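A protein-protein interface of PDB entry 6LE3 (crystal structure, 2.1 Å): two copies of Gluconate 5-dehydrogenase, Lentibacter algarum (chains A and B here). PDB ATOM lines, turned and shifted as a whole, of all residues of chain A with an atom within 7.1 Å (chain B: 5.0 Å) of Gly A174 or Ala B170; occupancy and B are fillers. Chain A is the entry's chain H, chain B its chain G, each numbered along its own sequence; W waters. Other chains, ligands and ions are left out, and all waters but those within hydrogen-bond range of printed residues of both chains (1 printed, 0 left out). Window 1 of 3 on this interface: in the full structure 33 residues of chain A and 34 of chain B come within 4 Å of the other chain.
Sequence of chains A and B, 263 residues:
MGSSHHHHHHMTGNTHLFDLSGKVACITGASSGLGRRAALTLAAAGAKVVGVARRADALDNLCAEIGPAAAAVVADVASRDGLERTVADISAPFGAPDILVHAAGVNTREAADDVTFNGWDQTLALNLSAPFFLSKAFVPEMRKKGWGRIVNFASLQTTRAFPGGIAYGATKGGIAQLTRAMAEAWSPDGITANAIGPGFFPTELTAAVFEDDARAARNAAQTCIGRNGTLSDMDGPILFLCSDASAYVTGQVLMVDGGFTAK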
ATOM      1  N   ASN A 127     -19.176  27.314  10.477  1.00  0.00           N
ATOM      2  CA  ASN A 127     -20.348  26.473  10.715  1.00  0.00           C
ATOM      3  C   ASN A 127     -20.003  25.012  10.993  1.00  0.00           C
ATOM      4  O   ASN A 127     -20.788  24.308  11.636  1.00  0.00           O
ATOM      5  CB  ASN A 127     -21.293  26.510   9.507  1.00  0.00           C
ATOM      6  CG  ASN A 127     -21.965  27.878   9.289  1.00  0.00           C
ATOM      7  OD1 ASN A 127     -21.644  28.869   9.944  1.00  0.00           O
ATOM      8  ND2 ASN A 127     -22.908  27.917   8.358  1.00  0.00           N
ATOM      9  N   LEU A 128     -18.881  24.522  10.487  1.00  0.00           N
ATOM     10  CA  LEU A 128     -18.535  23.104  10.568  1.00  0.00           C
ATOM     11  C   LEU A 128     -17.269  22.866  11.374  1.00  0.00           C
ATOM     12  O   LEU A 128     -17.302  22.122  12.368  1.00  0.00           O
ATOM     13  CB  LEU A 128     -18.391  22.521   9.145  1.00  0.00           C
ATOM     14  CG  LEU A 128     -18.611  21.016   8.886  1.00  0.00           C
ATOM     15  CD1 LEU A 128     -19.900  20.519   9.540  1.00  0.00           C
ATOM     16  CD2 LEU A 128     -18.602  20.666   7.356  1.00  0.00           C
ATOM     17  N   GLN A 157     -32.187  24.210   6.155  1.00  0.00           N
ATOM     18  CA  GLN A 157     -31.295  23.839   5.068  1.00  0.00           C
ATOM     19  C   GLN A 157     -30.400  22.662   5.434  1.00  0.00           C
ATOM     20  O   GLN A 157     -29.470  22.352   4.691  1.00  0.00           O
ATOM     21  CB  GLN A 157     -30.465  25.045   4.617  1.00  0.00           C
ATOM     22  CG  GLN A 157     -31.342  26.251   4.269  1.00  0.00           C
ATOM     23  CD  GLN A 157     -30.746  27.135   3.209  1.00  0.00           C
ATOM     24  OE1 GLN A 157     -30.538  26.706   2.064  1.00  0.00           O
ATOM     25  NE2 GLN A 157     -30.475  28.381   3.570  1.00  0.00           N
ATOM     26  N   THR A 158     -30.644  22.008   6.571  1.00  0.00           N
ATOM     27  CA  THR A 158     -30.093  20.670   6.747  1.00  0.00           C
ATOM     28  C   THR A 158     -30.718  19.686   5.758  1.00  0.00           C
ATOM     29  O   THR A 158     -30.060  18.732   5.340  1.00  0.00           O
ATOM     30  CB  THR A 158     -30.290  20.231   8.195  1.00  0.00           C
ATOM     31  OG1 THR A 158     -29.470  21.073   9.025  1.00  0.00           O
ATOM     32  CG2 THR A 158     -29.924  18.754   8.406  1.00  0.00           C
ATOM     33  N   TYR A 168     -23.941  27.291   2.902  1.00  0.00           N
ATOM     34  CA  TYR A 168     -24.641  27.162   4.175  1.00  0.00           C
ATOM     35  C   TYR A 168     -25.277  25.790   4.285  1.00  0.00           C
ATOM     36  O   TYR A 168     -25.102  25.089   5.289  1.00  0.00           O
ATOM     37  CB  TYR A 168     -25.689  28.270   4.287  1.00  0.00           C
ATOM     38  CG  TYR A 168     -26.419  28.341   5.596  1.00  0.00           C
ATOM     39  CD1 TYR A 168     -25.787  28.811   6.736  1.00  0.00           C
ATOM     40  CD2 TYR A 168     -27.758  27.936   5.690  1.00  0.00           C
ATOM     41  CE1 TYR A 168     -26.458  28.870   7.942  1.00  0.00           C
ATOM     42  CE2 TYR A 168     -28.440  27.996   6.895  1.00  0.00           C
ATOM     43  CZ  TYR A 168     -27.781  28.472   8.010  1.00  0.00           C
ATOM     44  OH  TYR A 168     -28.435  28.539   9.201  1.00  0.00           O
ATOM     45  N   GLY A 169     -26.003  25.384   3.245  1.00  0.00           N
ATOM     46  CA  GLY A 169     -26.607  24.067   3.248  1.00  0.00           C
ATOM     47  C   GLY A 169     -25.573  22.972   3.388  1.00  0.00           C
ATOM     48  O   GLY A 169     -25.777  22.011   4.124  1.00  0.00           O
ATOM     49  N   ALA A 170     -24.443  23.102   2.692  1.00  0.00           N
ATOM     50  CA  ALA A 170     -23.407  22.094   2.823  1.00  0.00           C
ATOM     51  C   ALA A 170     -23.013  21.934   4.279  1.00  0.00           C
ATOM     52  O   ALA A 170     -22.982  20.819   4.801  1.00  0.00           O
ATOM     53  CB  ALA A 170     -22.202  22.454   1.954  1.00  0.00           C
ATOM     54  N   THR A 171     -22.767  23.052   4.969  1.00  0.00           N
ATOM     55  CA  THR A 171     -22.319  22.954   6.358  1.00  0.00           C
ATOM     56  C   THR A 171     -23.424  22.466   7.295  1.00  0.00           C
ATOM     57  O   THR A 171     -23.131  21.822   8.308  1.00  0.00           O
ATOM     58  CB  THR A 171     -21.769  24.301   6.846  1.00  0.00           C
ATOM     59  OG1 THR A 171     -22.818  25.277   6.904  1.00  0.00           O
ATOM     60  CG2 THR A 171     -20.669  24.780   5.907  1.00  0.00           C
ATOM     61  N   LYS A 172     -24.692  22.753   6.980  1.00  0.00           N
ATOM     62  CA  LYS A 172     -25.788  22.357   7.866  1.00  0.00           C
ATOM     63  C   LYS A 172     -26.180  20.898   7.670  1.00  0.00           C
ATOM     64  O   LYS A 172     -26.625  20.255   8.617  1.00  0.00           O
ATOM     65  CB  LYS A 172     -27.005  23.254   7.639  1.00  0.00           C
ATOM     66  CG  LYS A 172     -26.852  24.676   8.205  1.00  0.00           C
ATOM     67  CD  LYS A 172     -26.047  24.682   9.497  1.00  0.00           C
ATOM     68  CE  LYS A 172     -26.233  25.964  10.258  1.00  0.00           C
ATOM     69  NZ  LYS A 172     -25.503  25.956  11.560  1.00  0.00           N
ATOM     70  N   GLY A 173     -26.059  20.372   6.450  1.00  0.00           N
ATOM     71  CA  GLY A 173     -26.085  18.932   6.271  1.00  0.00           C
ATOM     72  C   GLY A 173     -24.896  18.272   6.939  1.00  0.00           C
ATOM     73  O   GLY A 173     -25.004  17.170   7.476  1.00  0.00           O
ATOM     74  N   GLY A 174     -23.735  18.939   6.903  1.00  0.00           N
ATOM     75  CA  GLY A 174     -22.582  18.425   7.611  1.00  0.00           C
ATOM     76  C   GLY A 174     -22.808  18.348   9.111  1.00  0.00           C
ATOM     77  O   GLY A 174     -22.380  17.389   9.753  1.00  0.00           O
ATOM     78  N   ILE A 175     -23.486  19.359   9.680  1.00  0.00           N
ATOM     79  CA  ILE A 175     -23.692  19.432  11.129  1.00  0.00           C
ATOM     80  C   ILE A 175     -24.502  18.242  11.638  1.00  0.00           C
ATOM     81  O   ILE A 175     -24.256  17.735  12.733  1.00  0.00           O
ATOM     82  CB  ILE A 175     -24.342  20.778  11.505  1.00  0.00           C
ATOM     83  CG1 ILE A 175     -23.246  21.812  11.676  1.00  0.00           C
ATOM     84  CG2 ILE A 175     -25.117  20.676  12.831  1.00  0.00           C
ATOM     85  CD1 ILE A 175     -22.315  21.458  12.812  1.00  0.00           C
ATOM     86  N   ALA A 176     -25.463  17.776  10.849  1.00  0.00           N
ATOM     87  CA  ALA A 176     -26.241  16.589  11.196  1.00  0.00           C
ATOM     88  C   ALA A 176     -25.355  15.349  11.409  1.00  0.00           C
ATOM     89  O   ALA A 176     -25.414  14.676  12.461  1.00  0.00           O
ATOM     90  CB  ALA A 176     -27.268  16.348  10.090  1.00  0.00           C
ATOM     91  N   GLN A 177     -24.535  15.012  10.412  1.00  0.00           N
ATOM     92  CA  GLN A 177     -23.670  13.846  10.580  1.00  0.00           C
ATOM     93  C   GLN A 177     -22.576  14.103  11.604  1.00  0.00           C
ATOM     94  O   GLN A 177     -22.123  13.171  12.287  1.00  0.00           O
ATOM     95  CB  GLN A 177     -23.027  13.432   9.260  1.00  0.00           C
ATOM     96  CG  GLN A 177     -22.146  12.224   9.407  1.00  0.00           C
ATOM     97  CD  GLN A 177     -22.905  10.990   9.831  1.00  0.00           C
ATOM     98  OE1 GLN A 177     -24.116  10.877   9.598  1.00  0.00           O
ATOM     99  NE2 GLN A 177     -22.195  10.041  10.437  1.00  0.00           N
ATOM    100  N   LEU A 178     -22.108  15.341  11.692  1.00  0.00           N
ATOM    101  CA  LEU A 178     -21.131  15.680  12.711  1.00  0.00           C
ATOM    102  C   LEU A 178     -21.699  15.445  14.104  1.00  0.00           C
ATOM    103  O   LEU A 178     -20.991  14.972  15.001  1.00  0.00           O
ATOM    104  CB  LEU A 178     -20.697  17.139  12.537  1.00  0.00           C
ATOM    105  CG  LEU A 178     -19.569  17.584  13.471  1.00  0.00           C
ATOM    106  CD1 LEU A 178     -18.320  16.728  13.229  1.00  0.00           C
ATOM    107  CD2 LEU A 178     -19.256  19.064  13.273  1.00  0.00           C
ATOM    108  N   THR A 179     -22.973  15.805  14.305  1.00  0.00           N
ATOM    109  CA  THR A 179     -23.649  15.581  15.574  1.00  0.00           C
ATOM    110  C   THR A 179     -23.718  14.092  15.887  1.00  0.00           C
ATOM    111  O   THR A 179     -23.359  13.665  16.989  1.00  0.00           O
ATOM    112  CB  THR A 179     -25.045  16.211  15.532  1.00  0.00           C
ATOM    113  OG1 THR A 179     -24.929  17.618  15.286  1.00  0.00           O
ATOM    114  CG2 THR A 179     -25.736  16.052  16.866  1.00  0.00           C
ATOM    115  N   ARG A 180     -24.112  13.282  14.898  1.00  0.00           N
ATOM    116  CA  ARG A 180     -24.080  11.826  15.084  1.00  0.00           C
ATOM    117  C   ARG A 180     -22.667  11.326  15.413  1.00  0.00           C
ATOM    118  O   ARG A 180     -22.490  10.470  16.284  1.00  0.00           O
ATOM    119  CB  ARG A 180     -24.619  11.111  13.833  1.00  0.00           C
ATOM    120  CG  ARG A 180     -26.139  11.233  13.586  1.00  0.00           C
ATOM    121  CD  ARG A 180     -26.494  10.827  12.124  1.00  0.00           C
ATOM    122  NE  ARG A 180     -27.681  11.559  11.722  1.00  0.00           N
ATOM    123  CZ  ARG A 180     -27.815  12.312  10.642  1.00  0.00           C
ATOM    124  NH1 ARG A 180     -26.851  12.422   9.715  1.00  0.00           N
ATOM    125  NH2 ARG A 180     -28.968  12.927  10.476  1.00  0.00           N
ATOM    126  N   ALA A 181     -21.651  11.836  14.709  1.00  0.00           N
ATOM    127  CA  ALA A 181     -20.275  11.402  14.941  1.00  0.00           C
ATOM    128  C   ALA A 181     -19.799  11.754  16.341  1.00  0.00           C
ATOM    129  O   ALA A 181     -19.117  10.957  16.988  1.00  0.00           O
ATOM    130  CB  ALA A 181     -19.351  12.019  13.895  1.00  0.00           C
ATOM    131  N   TRP B 120      -8.312  16.911   9.049  1.00  0.00           N
ATOM    132  CA  TRP B 120      -9.626  17.532   8.882  1.00  0.00           C
ATOM    133  C   TRP B 120      -9.687  18.376   7.616  1.00  0.00           C
ATOM    134  O   TRP B 120     -10.580  18.191   6.783  1.00  0.00           O
ATOM    135  CB  TRP B 120      -9.952  18.372  10.114  1.00  0.00           C
ATOM    136  CG  TRP B 120     -11.247  19.148  10.053  1.00  0.00           C
ATOM    137  CD1 TRP B 120     -11.434  20.409   9.521  1.00  0.00           C
ATOM    138  CD2 TRP B 120     -12.522  18.740  10.577  1.00  0.00           C
ATOM    139  NE1 TRP B 120     -12.748  20.785   9.673  1.00  0.00           N
ATOM    140  CE2 TRP B 120     -13.436  19.784  10.313  1.00  0.00           C
ATOM    141  CE3 TRP B 120     -12.983  17.588  11.232  1.00  0.00           C
ATOM    142  CZ2 TRP B 120     -14.783  19.718  10.697  1.00  0.00           C
ATOM    143  CZ3 TRP B 120     -14.330  17.516  11.599  1.00  0.00           C
ATOM    144  CH2 TRP B 120     -15.207  18.579  11.339  1.00  0.00           C
ATOM    145  N   GLY B 165     -14.612   8.013  11.840  1.00  0.00           N
ATOM    146  CA  GLY B 165     -15.097   8.712  10.662  1.00  0.00           C
ATOM    147  C   GLY B 165     -15.611  10.131  10.822  1.00  0.00           C
ATOM    148  O   GLY B 165     -16.371  10.584   9.968  1.00  0.00           O
ATOM    149  N   ILE B 166     -15.221  10.857  11.875  1.00  0.00           N
ATOM    150  CA  ILE B 166     -15.908  12.113  12.183  1.00  0.00           C
ATOM    151  C   ILE B 166     -15.736  13.142  11.051  1.00  0.00           C
ATOM    152  O   ILE B 166     -16.717  13.743  10.593  1.00  0.00           O
ATOM    153  CB  ILE B 166     -15.474  12.649  13.564  1.00  0.00           C
ATOM    154  CG1 ILE B 166     -16.262  13.911  13.938  1.00  0.00           C
ATOM    155  CG2 ILE B 166     -13.964  12.853  13.666  1.00  0.00           C
ATOM    156  CD1 ILE B 166     -16.590  14.018  15.443  1.00  0.00           C
ATOM    157  N   ALA B 167     -14.510  13.348  10.562  1.00  0.00           N
ATOM    158  CA  ALA B 167     -14.318  14.277   9.443  1.00  0.00           C
ATOM    159  C   ALA B 167     -15.002  13.772   8.181  1.00  0.00           C
ATOM    160  O   ALA B 167     -15.738  14.513   7.506  1.00  0.00           O
ATOM    161  CB  ALA B 167     -12.826  14.490   9.173  1.00  0.00           C
ATOM    162  N   TYR B 168     -14.756  12.503   7.851  1.00  0.00           N
ATOM    163  CA  TYR B 168     -15.373  11.885   6.686  1.00  0.00           C
ATOM    164  C   TYR B 168     -16.892  11.996   6.768  1.00  0.00           C
ATOM    165  O   TYR B 168     -17.552  12.412   5.809  1.00  0.00           O
ATOM    166  CB  TYR B 168     -14.918  10.426   6.607  1.00  0.00           C
ATOM    167  CG  TYR B 168     -15.421   9.662   5.425  1.00  0.00           C
ATOM    168  CD1 TYR B 168     -14.944   9.935   4.150  1.00  0.00           C
ATOM    169  CD2 TYR B 168     -16.369   8.648   5.582  1.00  0.00           C
ATOM    170  CE1 TYR B 168     -15.398   9.240   3.064  1.00  0.00           C
ATOM    171  CE2 TYR B 168     -16.829   7.935   4.488  1.00  0.00           C
ATOM    172  CZ  TYR B 168     -16.329   8.240   3.236  1.00  0.00           C
ATOM    173  OH  TYR B 168     -16.766   7.565   2.140  1.00  0.00           O
ATOM    174  N   GLY B 169     -17.461  11.640   7.922  1.00  0.00           N
ATOM    175  CA  GLY B 169     -18.899  11.756   8.096  1.00  0.00           C
ATOM    176  C   GLY B 169     -19.399  13.176   7.943  1.00  0.00           C
ATOM    177  O   GLY B 169     -20.440  13.414   7.337  1.00  0.00           O
ATOM    178  N   ALA B 170     -18.674  14.140   8.498  1.00  0.00           N
ATOM    179  CA  ALA B 170     -19.086  15.522   8.324  1.00  0.00           C
ATOM    180  C   ALA B 170     -19.219  15.847   6.848  1.00  0.00           C
ATOM    181  O   ALA B 170     -20.236  16.401   6.414  1.00  0.00           O
ATOM    182  CB  ALA B 170     -18.096  16.461   9.010  1.00  0.00           C
ATOM    183  N   THR B 171     -18.212  15.465   6.049  1.00  0.00           N
ATOM    184  CA  THR B 171     -18.252  15.805   4.624  1.00  0.00           C
ATOM    185  C   THR B 171     -19.313  15.004   3.868  1.00  0.00           C
ATOM    186  O   THR B 171     -19.856  15.484   2.870  1.00  0.00           O
ATOM    187  CB  THR B 171     -16.883  15.597   3.950  1.00  0.00           C
ATOM    188  OG1 THR B 171     -16.573  14.193   3.878  1.00  0.00           O
ATOM    189  CG2 THR B 171     -15.787  16.339   4.688  1.00  0.00           C
ATOM    190  N   LYS B 172     -19.619  13.790   4.309  1.00  0.00           N
ATOM    191  CA  LYS B 172     -20.603  12.990   3.576  1.00  0.00           C
ATOM    192  C   LYS B 172     -22.030  13.377   3.945  1.00  0.00           C
ATOM    193  O   LYS B 172     -22.932  13.243   3.115  1.00  0.00           O
ATOM    194  CB  LYS B 172     -20.379  11.500   3.829  1.00  0.00           C
ATOM    195  CG  LYS B 172     -19.141  10.941   3.144  1.00  0.00           C
ATOM    196  CD  LYS B 172     -18.898  11.572   1.800  1.00  0.00           C
ATOM    197  CE  LYS B 172     -17.958  10.714   0.979  1.00  0.00           C
ATOM    198  NZ  LYS B 172     -17.748  11.212  -0.421  1.00  0.00           N
ATOM    199  N   GLY B 173     -22.263  13.825   5.182  1.00  0.00           N
ATOM    200  CA  GLY B 173     -23.498  14.520   5.465  1.00  0.00           C
ATOM    201  C   GLY B 173     -23.595  15.808   4.672  1.00  0.00           C
ATOM    202  O   GLY B 173     -24.660  16.154   4.154  1.00  0.00           O
ATOM    203  N   GLY B 174     -22.465  16.509   4.520  1.00  0.00           N
ATOM    204  CA  GLY B 174     -22.445  17.712   3.706  1.00  0.00           C
ATOM    205  C   GLY B 174     -22.789  17.442   2.252  1.00  0.00           C
ATOM    206  O   GLY B 174     -23.484  18.237   1.620  1.00  0.00           O
HETATM  207  O   HOH W   1     -19.435   9.835  10.627  1.00  0.00           O
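The side-chain amide oxygen (OE1) of Gln A177 is in hydrogen-bond range of the guanidinium group (NH1) of Arg A180 (3.1 Å).
Water W1 lies within hydrogen-bond range of the side-chain amide nitrogen (NE2) of Gln A177 (2.8 Å) and the backbone carbonyl oxygen (O) of Gly B165 (3.2 Å).
Ala A170 touches Gly B174, and with the chains exchanged Gly A174 touches Ala B170.
Gly B173 touches its own counterpart, Gly A173.
Gly A173 touches Gly B174, and with the chains exchanged Gly A174 touches Gly B173.
Gly B174 touches its own counterpart, Gly A174.
Of the 11 pairs that touch across the chains among the printed residues, 6 have their exchanged pair printed and touching as well.
Of the 11 printed residues of chain B, 6 touch a printed residue of chain A.
Hydrophobic or aromatic side chains of chain B within 4 Å of the printed part of chain A: Trp B120 and Ile B166.
Of the 18 printed residues of chain A, 7 touch a printed residue of chain B.
Hydrophobic or aromatic side chains of chain A that line the printed part of chain B: Leu A178 and Ala A181.
Printed residues of chain B within 4 Å of Gly A173: Gly B173 (3.4 Å) and Gly B174 (3.9 Å).
Gly A174 touches just these residues of chain B: Ala B170 (3.3 Å), Gly B173 (3.8 Å) and Gly B174 (3.6 Å).
Printed residues of chain B within 4 Å of Leu A178: Ile B166.
Thr A179 touches none of the printed residues of chain B.
Printed residues of chain B within 4 Å of Ala A181: Ile B166.
Printed residues of chain A within 4 Å of Trp B120: Leu A128.
Tyr B168 touches none of the printed residues of chain A.
Gly B169 touches just one residue of chain A: Gln A177 (2.9 Å).
Printed residues of chain A within 4 Å of Ala B170: Gly A174.
O of Gly A173 sits close to O of Gly B173.
Among the printed residues, pairs that only touch across the chains: Gln A177 with Gly B169 (2.9 Å), Gly A174 with Ala B170 (3.3 Å), Ala A170 with Gly B174 (3.3 Å), Leu A178 with Ile B166 (3.6 Å), Ala A181 with Ile B166 (3.6 Å), Gly A174 with Gly B174 (3.6 Å), Gly A174 with Gly B173 (3.8 Å), Gly A173 with Gly B174 (3.9 Å), Leu A128 with Trp B120 (3.9 Å) and Gln A177 with Gly B173 (3.98 Å).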
